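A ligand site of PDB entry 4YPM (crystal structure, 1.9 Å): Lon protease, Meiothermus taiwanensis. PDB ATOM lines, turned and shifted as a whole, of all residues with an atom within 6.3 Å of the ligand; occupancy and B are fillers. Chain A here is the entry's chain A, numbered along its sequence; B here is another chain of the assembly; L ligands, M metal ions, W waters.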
ATOM      1  N   GLY A 109      19.051 -28.942  -6.258  1.00  0.00           N
ATOM      2  CA  GLY A 109      20.314 -28.370  -6.689  1.00  0.00           C
ATOM      3  C   GLY A 109      20.982 -29.275  -7.708  1.00  0.00           C
ATOM      4  O   GLY A 109      20.475 -30.363  -8.021  1.00  0.00           O
ATOM      5  N   LEU A 110      22.110 -28.817  -8.230  1.00  0.00           N
ATOM      6  CA  LEU A 110      22.799 -29.481  -9.334  1.00  0.00           C
ATOM      7  C   LEU A 110      24.303 -29.385  -9.072  1.00  0.00           C
ATOM      8  O   LEU A 110      24.822 -28.318  -8.782  1.00  0.00           O
ATOM      9  CB  LEU A 110      22.472 -28.787 -10.661  1.00  0.00           C
ATOM     10  CG  LEU A 110      21.003 -28.723 -11.112  1.00  0.00           C
ATOM     11  CD1 LEU A 110      20.800 -27.641 -12.151  1.00  0.00           C
ATOM     12  CD2 LEU A 110      20.547 -30.085 -11.587  1.00  0.00           C
ATOM     13  N   ALA A 111      24.982 -30.524  -9.177  1.00  0.00           N
ATOM     14  CA  ALA A 111      26.422 -30.581  -8.937  1.00  0.00           C
ATOM     15  C   ALA A 111      27.107 -31.167 -10.163  1.00  0.00           C
ATOM     16  O   ALA A 111      26.475 -31.782 -11.029  1.00  0.00           O
ATOM     17  CB  ALA A 111      26.729 -31.419  -7.710  1.00  0.00           C
ATOM     18  N   TRP A 112      28.420 -30.994 -10.235  1.00  0.00           N
ATOM     19  CA  TRP A 112      29.159 -31.661 -11.289  1.00  0.00           C
ATOM     20  C   TRP A 112      30.503 -32.169 -10.900  1.00  0.00           C
ATOM     21  O   TRP A 112      31.040 -31.811  -9.852  1.00  0.00           O
ATOM     22  CB  TRP A 112      29.250 -30.799 -12.517  1.00  0.00           C
ATOM     23  CG  TRP A 112      30.239 -29.674 -12.528  1.00  0.00           C
ATOM     24  CD1 TRP A 112      30.377 -28.679 -11.622  1.00  0.00           C
ATOM     25  CD2 TRP A 112      31.183 -29.399 -13.577  1.00  0.00           C
ATOM     26  NE1 TRP A 112      31.356 -27.780 -12.041  1.00  0.00           N
ATOM     27  CE2 TRP A 112      31.868 -28.216 -13.229  1.00  0.00           C
ATOM     28  CE3 TRP A 112      31.496 -30.025 -14.773  1.00  0.00           C
ATOM     29  CZ2 TRP A 112      32.850 -27.659 -14.041  1.00  0.00           C
ATOM     30  CZ3 TRP A 112      32.480 -29.478 -15.575  1.00  0.00           C
ATOM     31  CH2 TRP A 112      33.135 -28.301 -15.207  1.00  0.00           C
ATOM     32  N   THR A 113      31.007 -33.059 -11.746  1.00  0.00           N
ATOM     33  CA  THR A 113      32.295 -33.703 -11.566  1.00  0.00           C
ATOM     34  C   THR A 113      32.916 -33.804 -12.960  1.00  0.00           C
ATOM     35  O   THR A 113      32.278 -33.454 -13.957  1.00  0.00           O
ATOM     36  CB  THR A 113      32.158 -35.125 -11.014  1.00  0.00           C
ATOM     37  OG1 THR A 113      31.639 -35.975 -12.045  1.00  0.00           O
ATOM     38  CG2 THR A 113      31.220 -35.170  -9.785  1.00  0.00           C
ATOM     39  N   GLY A 116      30.469 -35.856 -15.233  1.00  0.00           N
ATOM     40  CA  GLY A 116      29.091 -35.459 -15.525  1.00  0.00           C
ATOM     41  C   GLY A 116      28.417 -34.746 -14.365  1.00  0.00           C
ATOM     42  O   GLY A 116      29.070 -34.385 -13.384  1.00  0.00           O
ATOM     43  N   GLY A 117      27.114 -34.540 -14.500  1.00  0.00           N
ATOM     44  CA  GLY A 117      26.324 -33.818 -13.503  1.00  0.00           C
ATOM     45  C   GLY A 117      25.500 -34.745 -12.633  1.00  0.00           C
ATOM     46  O   GLY A 117      25.297 -35.913 -12.956  1.00  0.00           O
ATOM     47  N   THR A 118      25.004 -34.198 -11.529  1.00  0.00           N
ATOM     48  CA  THR A 118      24.269 -34.955 -10.543  1.00  0.00           C
ATOM     49  C   THR A 118      23.217 -34.019  -9.915  1.00  0.00           C
ATOM     50  O   THR A 118      23.537 -32.921  -9.510  1.00  0.00           O
ATOM     51  CB  THR A 118      25.206 -35.456  -9.415  1.00  0.00           C
ATOM     52  OG1 THR A 118      26.262 -36.246  -9.969  1.00  0.00           O
ATOM     53  CG2 THR A 118      24.483 -36.291  -8.409  1.00  0.00           C
ATOM     54  N   LEU A 120      21.166 -32.995  -6.712  1.00  0.00           N
ATOM     55  CA  LEU A 120      21.313 -33.130  -5.248  1.00  0.00           C
ATOM     56  C   LEU A 120      20.200 -32.320  -4.604  1.00  0.00           C
ATOM     57  O   LEU A 120      19.957 -31.202  -5.005  1.00  0.00           O
ATOM     58  CB  LEU A 120      22.653 -32.572  -4.736  1.00  0.00           C
ATOM     59  CG  LEU A 120      23.962 -33.245  -5.133  1.00  0.00           C
ATOM     60  CD1 LEU A 120      25.126 -32.462  -4.549  1.00  0.00           C
ATOM     61  CD2 LEU A 120      24.004 -34.688  -4.693  1.00  0.00           C
ATOM     62  N   ILE A 122      18.806 -30.281  -1.419  1.00  0.00           N
ATOM     63  CA  ILE A 122      19.191 -29.592  -0.205  1.00  0.00           C
ATOM     64  C   ILE A 122      18.001 -29.708   0.762  1.00  0.00           C
ATOM     65  O   ILE A 122      16.871 -29.404   0.376  1.00  0.00           O
ATOM     66  CB  ILE A 122      19.574 -28.137  -0.471  1.00  0.00           C
ATOM     67  CG1 ILE A 122      20.932 -28.020  -1.213  1.00  0.00           C
ATOM     68  CG2 ILE A 122      19.726 -27.395   0.834  1.00  0.00           C
ATOM     69  CD1 ILE A 122      21.040 -28.823  -2.471  1.00  0.00           C
ATOM     70  N   VAL A 142      33.990 -23.798   1.734  1.00  0.00           N
ATOM     71  CA  VAL A 142      33.348 -22.857   0.808  1.00  0.00           C
ATOM     72  C   VAL A 142      31.819 -23.042   0.783  1.00  0.00           C
ATOM     73  O   VAL A 142      31.043 -22.069   0.778  1.00  0.00           O
ATOM     74  CB  VAL A 142      33.939 -23.005  -0.608  1.00  0.00           C
ATOM     75  CG1 VAL A 142      33.080 -22.276  -1.642  1.00  0.00           C
ATOM     76  CG2 VAL A 142      35.378 -22.467  -0.628  1.00  0.00           C
ATOM     77  N   MET A 143      31.361 -24.290   0.735  1.00  0.00           N
ATOM     78  CA  MET A 143      29.914 -24.529   0.733  1.00  0.00           C
ATOM     79  C   MET A 143      29.273 -24.111   2.056  1.00  0.00           C
ATOM     80  O   MET A 143      28.167 -23.572   2.092  1.00  0.00           O
ATOM     81  CB  MET A 143      29.620 -25.961   0.382  1.00  0.00           C
ATOM     82  CG  MET A 143      28.149 -26.278   0.206  1.00  0.00           C
ATOM     83  SD  MET A 143      28.000 -27.929  -0.499  1.00  0.00           S
ATOM     84  CE  MET A 143      26.216 -28.140  -0.439  1.00  0.00           C
ATOM     85  N   VAL A 177      22.730 -32.155   3.206  1.00  0.00           N
ATOM     86  CA  VAL A 177      22.740 -32.520   1.809  1.00  0.00           C
ATOM     87  C   VAL A 177      23.127 -33.979   1.672  1.00  0.00           C
ATOM     88  O   VAL A 177      24.304 -34.341   1.741  1.00  0.00           O
ATOM     89  CB  VAL A 177      23.659 -31.620   0.957  1.00  0.00           C
ATOM     90  CG1 VAL A 177      23.371 -31.857  -0.515  1.00  0.00           C
ATOM     91  CG2 VAL A 177      23.454 -30.158   1.299  1.00  0.00           C
ATOM     92  N   THR A 182      29.195 -38.758   0.958  1.00  0.00           N
ATOM     93  CA  THR A 182      29.860 -38.162  -0.217  1.00  0.00           C
ATOM     94  C   THR A 182      30.275 -36.718   0.065  1.00  0.00           C
ATOM     95  O   THR A 182      29.444 -35.882   0.385  1.00  0.00           O
ATOM     96  CB  THR A 182      28.926 -38.187  -1.431  1.00  0.00           C
ATOM     97  OG1 THR A 182      28.536 -39.546  -1.672  1.00  0.00           O
ATOM     98  CG2 THR A 182      29.608 -37.615  -2.693  1.00  0.00           C
ATOM     99  N   PRO A 183      31.576 -36.427  -0.059  1.00  0.00           N
ATOM    100  CA  PRO A 183      31.963 -35.029   0.091  1.00  0.00           C
ATOM    101  C   PRO A 183      31.369 -34.131  -0.958  1.00  0.00           C
ATOM    102  O   PRO A 183      31.245 -34.524  -2.109  1.00  0.00           O
ATOM    103  CB  PRO A 183      33.489 -35.072  -0.042  1.00  0.00           C
ATOM    104  CG  PRO A 183      33.853 -36.467   0.293  1.00  0.00           C
ATOM    105  CD  PRO A 183      32.745 -37.299  -0.249  1.00  0.00           C
ATOM    106  N   LYS A 184      30.999 -32.927  -0.545  1.00  0.00           N
ATOM    107  CA  LYS A 184      30.427 -31.917  -1.414  1.00  0.00           C
ATOM    108  C   LYS A 184      31.084 -30.577  -1.114  1.00  0.00           C
ATOM    109  O   LYS A 184      31.448 -30.293   0.019  1.00  0.00           O
ATOM    110  CB  LYS A 184      28.923 -31.792  -1.202  1.00  0.00           C
ATOM    111  CG  LYS A 184      28.231 -33.147  -1.188  1.00  0.00           C
ATOM    112  CD  LYS A 184      26.815 -33.083  -0.739  1.00  0.00           C
ATOM    113  CE  LYS A 184      26.295 -34.505  -0.680  1.00  0.00           C
ATOM    114  NZ  LYS A 184      26.730 -35.247   0.532  1.00  0.00           N
ATOM    115  N   ASP A 185      31.239 -29.747  -2.122  1.00  0.00           N
ATOM    116  CA  ASP A 185      31.802 -28.420  -1.881  1.00  0.00           C
ATOM    117  C   ASP A 185      31.436 -27.460  -3.006  1.00  0.00           C
ATOM    118  O   ASP A 185      30.881 -27.848  -4.020  1.00  0.00           O
ATOM    119  CB  ASP A 185      33.336 -28.500  -1.720  1.00  0.00           C
ATOM    120  CG  ASP A 185      33.903 -27.357  -0.907  1.00  0.00           C
ATOM    121  OD1 ASP A 185      33.151 -26.477  -0.404  1.00  0.00           O
ATOM    122  OD2 ASP A 185      35.150 -27.323  -0.756  1.00  0.00           O
ATOM    123  N   GLY A 186      31.725 -26.179  -2.766  1.00  0.00           N
ATOM    124  CA  GLY A 186      31.560 -25.141  -3.775  1.00  0.00           C
ATOM    125  C   GLY A 186      30.479 -24.128  -3.447  1.00  0.00           C
ATOM    126  O   GLY A 186      29.656 -24.364  -2.560  1.00  0.00           O
ATOM    127  N   PRO A 187      30.483 -22.985  -4.145  1.00  0.00           N
ATOM    128  CA  PRO A 187      29.574 -21.891  -3.816  1.00  0.00           C
ATOM    129  C   PRO A 187      28.273 -21.889  -4.619  1.00  0.00           C
ATOM    130  O   PRO A 187      27.435 -21.016  -4.411  1.00  0.00           O
ATOM    131  CB  PRO A 187      30.397 -20.663  -4.201  1.00  0.00           C
ATOM    132  CG  PRO A 187      31.173 -21.138  -5.391  1.00  0.00           C
ATOM    133  CD  PRO A 187      31.512 -22.564  -5.103  1.00  0.00           C
ATOM    134  N   SER A 188      28.112 -22.833  -5.540  1.00  0.00           N
ATOM    135  CA  SER A 188      27.026 -22.752  -6.541  1.00  0.00           C
ATOM    136  C   SER A 188      25.645 -23.192  -6.039  1.00  0.00           C
ATOM    137  O   SER A 188      24.681 -23.189  -6.816  1.00  0.00           O
ATOM    138  CB  SER A 188      27.400 -23.557  -7.774  1.00  0.00           C
ATOM    139  OG  SER A 188      27.301 -24.936  -7.498  1.00  0.00           O
ATOM    140  N   ALA A 189      25.550 -23.628  -4.796  1.00  0.00           N
ATOM    141  CA  ALA A 189      24.256 -23.932  -4.192  1.00  0.00           C
ATOM    142  C   ALA A 189      23.779 -22.794  -3.264  1.00  0.00           C
ATOM    143  O   ALA A 189      22.874 -22.996  -2.440  1.00  0.00           O
ATOM    144  CB  ALA A 189      24.330 -25.243  -3.444  1.00  0.00           C
ATOM    145  N   THR A 192      20.169 -22.205  -3.874  1.00  0.00           N
ATOM    146  CA  THR A 192      19.494 -23.426  -3.516  1.00  0.00           C
ATOM    147  C   THR A 192      19.323 -23.480  -2.008  1.00  0.00           C
ATOM    148  O   THR A 192      18.266 -23.805  -1.495  1.00  0.00           O
ATOM    149  CB  THR A 192      20.305 -24.641  -4.012  1.00  0.00           C
ATOM    150  OG1 THR A 192      20.852 -24.323  -5.296  1.00  0.00           O
ATOM    151  CG2 THR A 192      19.428 -25.887  -4.090  1.00  0.00           C
ATOM    152  N   THR A 213      20.911 -23.534  -9.901  1.00  0.00           N
ATOM    153  CA  THR A 213      22.329 -23.384  -9.611  1.00  0.00           C
ATOM    154  C   THR A 213      22.660 -21.895  -9.643  1.00  0.00           C
ATOM    155  O   THR A 213      22.181 -21.168 -10.498  1.00  0.00           O
ATOM    156  CB  THR A 213      23.205 -24.258 -10.561  1.00  0.00           C
ATOM    157  OG1 THR A 213      24.574 -24.253 -10.096  1.00  0.00           O
ATOM    158  CG2 THR A 213      23.145 -23.806 -12.025  1.00  0.00           C
ATOM    159  N   ILE A 225      28.295 -19.492 -12.273  1.00  0.00           N
ATOM    160  CA  ILE A 225      28.786 -20.776 -11.817  1.00  0.00           C
ATOM    161  C   ILE A 225      29.409 -21.545 -12.985  1.00  0.00           C
ATOM    162  O   ILE A 225      29.425 -21.080 -14.134  1.00  0.00           O
ATOM    163  CB  ILE A 225      27.649 -21.562 -11.108  1.00  0.00           C
ATOM    164  CG1 ILE A 225      26.350 -21.640 -11.921  1.00  0.00           C
ATOM    165  CG2 ILE A 225      27.308 -20.861  -9.824  1.00  0.00           C
ATOM    166  CD1 ILE A 225      26.394 -22.382 -13.238  1.00  0.00           C
ATOM    167  N   GLY A 226      29.916 -22.730 -12.675  1.00  0.00           N
ATOM    168  CA  GLY A 226      30.519 -23.624 -13.661  1.00  0.00           C
ATOM    169  C   GLY A 226      29.673 -24.857 -13.893  1.00  0.00           C
ATOM    170  O   GLY A 226      28.663 -25.112 -13.185  1.00  0.00           O
ATOM    171  N   GLY A 227      30.070 -25.620 -14.906  1.00  0.00           N
ATOM    172  CA  GLY A 227      29.439 -26.894 -15.204  1.00  0.00           C
ATOM    173  C   GLY A 227      28.021 -26.792 -15.745  1.00  0.00           C
ATOM    174  O   GLY A 227      27.212 -27.678 -15.514  1.00  0.00           O
ATOM    175  N   LYS A 231      25.307 -29.897 -15.622  1.00  0.00           N
ATOM    176  CA  LYS A 231      24.199 -29.711 -14.689  1.00  0.00           C
ATOM    177  C   LYS A 231      22.851 -29.761 -15.405  1.00  0.00           C
ATOM    178  O   LYS A 231      21.912 -30.404 -14.947  1.00  0.00           O
ATOM    179  CB  LYS A 231      24.366 -28.406 -13.950  1.00  0.00           C
ATOM    180  CG  LYS A 231      25.514 -28.400 -12.932  1.00  0.00           C
ATOM    181  CD  LYS A 231      25.742 -26.985 -12.417  1.00  0.00           C
ATOM    182  CE  LYS A 231      26.803 -26.958 -11.313  1.00  0.00           C
ATOM    183  NZ  LYS A 231      27.137 -25.565 -10.897  1.00  0.00           N
ATOM    184  N   ALA B 181      34.744 -18.809  -3.670  1.00  0.00           N
ATOM    185  CA  ALA B 181      35.791 -19.834  -3.722  1.00  0.00           C
ATOM    186  C   ALA B 181      37.241 -19.312  -3.678  1.00  0.00           C
ATOM    187  O   ALA B 181      38.147 -20.052  -3.310  1.00  0.00           O
ATOM    188  CB  ALA B 181      35.598 -20.708  -4.941  1.00  0.00           C
HETATM  189  N1  LIG L   1      29.502 -33.596  -7.245  1.00  0.00           N
HETATM  190  C1  LIG L   1      29.729 -33.139  -5.987  1.00  0.00           C
HETATM  191  C2  LIG L   1      29.280 -33.879  -4.890  1.00  0.00           C
HETATM  192  N2  LIG L   1      28.682 -35.070  -5.080  1.00  0.00           N
HETATM  193  C3  LIG L   1      28.478 -35.523  -6.328  1.00  0.00           C
HETATM  194  C4  LIG L   1      28.873 -34.760  -7.423  1.00  0.00           C
HETATM  195  C5  LIG L   1      30.318 -31.778  -5.796  1.00  0.00           C
HETATM  196  O1  LIG L   1      30.506 -31.349  -4.660  1.00  0.00           O
HETATM  197  N3  LIG L   1      30.526 -31.054  -6.889  1.00  0.00           N
HETATM  198  C6  LIG L   1      30.981 -29.674  -6.799  1.00  0.00           C
HETATM  199  C7  LIG L   1      32.182 -29.365  -7.715  1.00  0.00           C
HETATM  200  C8  LIG L   1      32.701 -27.972  -7.401  1.00  0.00           C
HETATM  201  C9  LIG L   1      33.573 -27.789  -6.321  1.00  0.00           C
HETATM  202  C10 LIG L   1      34.053 -26.505  -6.029  1.00  0.00           C
HETATM  203  C11 LIG L   1      33.641 -25.399  -6.777  1.00  0.00           C
HETATM  204  C12 LIG L   1      32.743 -25.579  -7.839  1.00  0.00           C
HETATM  205  C13 LIG L   1      32.300 -26.861  -8.156  1.00  0.00           C
HETATM  206  C14 LIG L   1      29.766 -28.871  -7.205  1.00  0.00           C
HETATM  207  O2  LIG L   1      29.312 -28.995  -8.344  1.00  0.00           O
HETATM  208  N4  LIG L   1      29.213 -28.078  -6.277  1.00  0.00           N
HETATM  209  C15 LIG L   1      28.032 -27.253  -6.545  1.00  0.00           C
HETATM  210  C16 LIG L   1      27.386 -26.956  -5.172  1.00  0.00           C
HETATM  211  C17 LIG L   1      26.580 -28.100  -4.534  1.00  0.00           C
HETATM  212  C18 LIG L   1      25.332 -28.448  -5.364  1.00  0.00           C
HETATM  213  C19 LIG L   1      27.384 -29.334  -4.140  1.00  0.00           C
HETATM  214  B1  LIG L   1      28.500 -25.909  -7.331  1.00  0.00           B
HETATM  215  O3  LIG L   1      28.869 -26.052  -8.826  1.00  0.00           O
HETATM  216  O4  LIG L   1      29.555 -25.003  -6.695  1.00  0.00           O
HETATM  217 MG    MG M   1      24.881 -25.804  -8.002  1.00  0.00          MG
HETATM  218  O   HOH W   1      32.410 -25.442 -11.339  1.00  0.00           O
HETATM  219  O   HOH W   2      30.246 -23.974 -10.124  1.00  0.00           O
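Water W2 bridges an oxygen (O3) of the ligand (2.8 Å) and the backbone NH of Gly 226 (2.9 Å).
The side-chain amino group of Lys 231 lies within hydrogen-bond range of an oxygen (O3) of the ligand (2.7 Å).
OG of Ser 188 is covalently linked to B1 of the ligand (1.6 Å).
O of Asp 185 is in hydrogen-bond range of N4 of the ligand (2.8 Å).
The backbone NH (N) of Asp 185 lies within hydrogen-bond range of an oxygen (O1) of the ligand.
The backbone NH (N) of Ser 188 lies close to an oxygen (O4) of the ligand (2.9 Å).
The backbone carbonyl oxygen of Trp 112 is in hydrogen-bond range of a nitrogen (N3) of the ligand, 3.1 Å away.
N of Trp 112 is in hydrogen-bond range of O2 of the ligand (2.9 Å).
NZ of Lys 231 is in hydrogen-bond range of OG1 of Thr 213 (3.0 Å).
The backbone carbonyl oxygen (O) of Ser 188 is in hydrogen-bond range of the side-chain hydroxyl (OG1) of Thr 213 (3.4 Å).
O of Gly 116 sits at hydrogen-bond distance from OG1 of Thr 113 (3.3 Å).
The backbone carbonyl oxygen of Thr 118 lies within hydrogen-bond range of the backbone NH of Ala 111 (2.8 Å).
The backbone NH (N) of Gly 109 sits at hydrogen-bond distance from the backbone carbonyl oxygen (O) of Leu 120 (2.7 Å).
NZ of Lys 231 lies within hydrogen-bond range of OG of Ser 188 (3.5 Å).
NZ of Lys 184 is in hydrogen-bond range of O of Thr 182 (2.8 Å).
The side-chain amino group (NZ) of Lys 231 lies within hydrogen-bond range of the backbone carbonyl oxygen (O) of Gly 226, at 2.8 Å.
O4 of the ligand sits close to N of Pro 187, 3.4 Å away.
Leu 110 touches the ligand.
Ala 111 touches the ligand (CA to O2, 3.3 Å).
CG2 of Thr 113 touches C4 of the ligand (3.4 Å).
Thr 118 touches the ligand (OG1 to C4, 3.9 Å).
Leu 120 touches the ligand.
Met 143 touches the ligand (SD to C19, 3.95 Å).
Thr 182 touches the ligand.
Pro 183 touches the ligand (O to C2, 3.5 Å).
Lys 184 touches the ligand.
C of Gly 186 touches O4 of the ligand, at 3.5 Å.
Ala 189 touches the ligand.
Hydrophobic or aromatic side chains within 4 Å of the ligand: Ala 111, Trp 112, Leu 120, Met 143, Pro 187 and Ala 189.
16 residues have an atom within 4 Å of the ligand: Leu 110, Ala 111, Trp 112, Thr 113, Thr 118, Leu 120, Met 143, Thr 182, Pro 183, Lys 184, Asp 185, Gly 186, Pro 187, Ser 188, Ala 189 and Lys 231.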
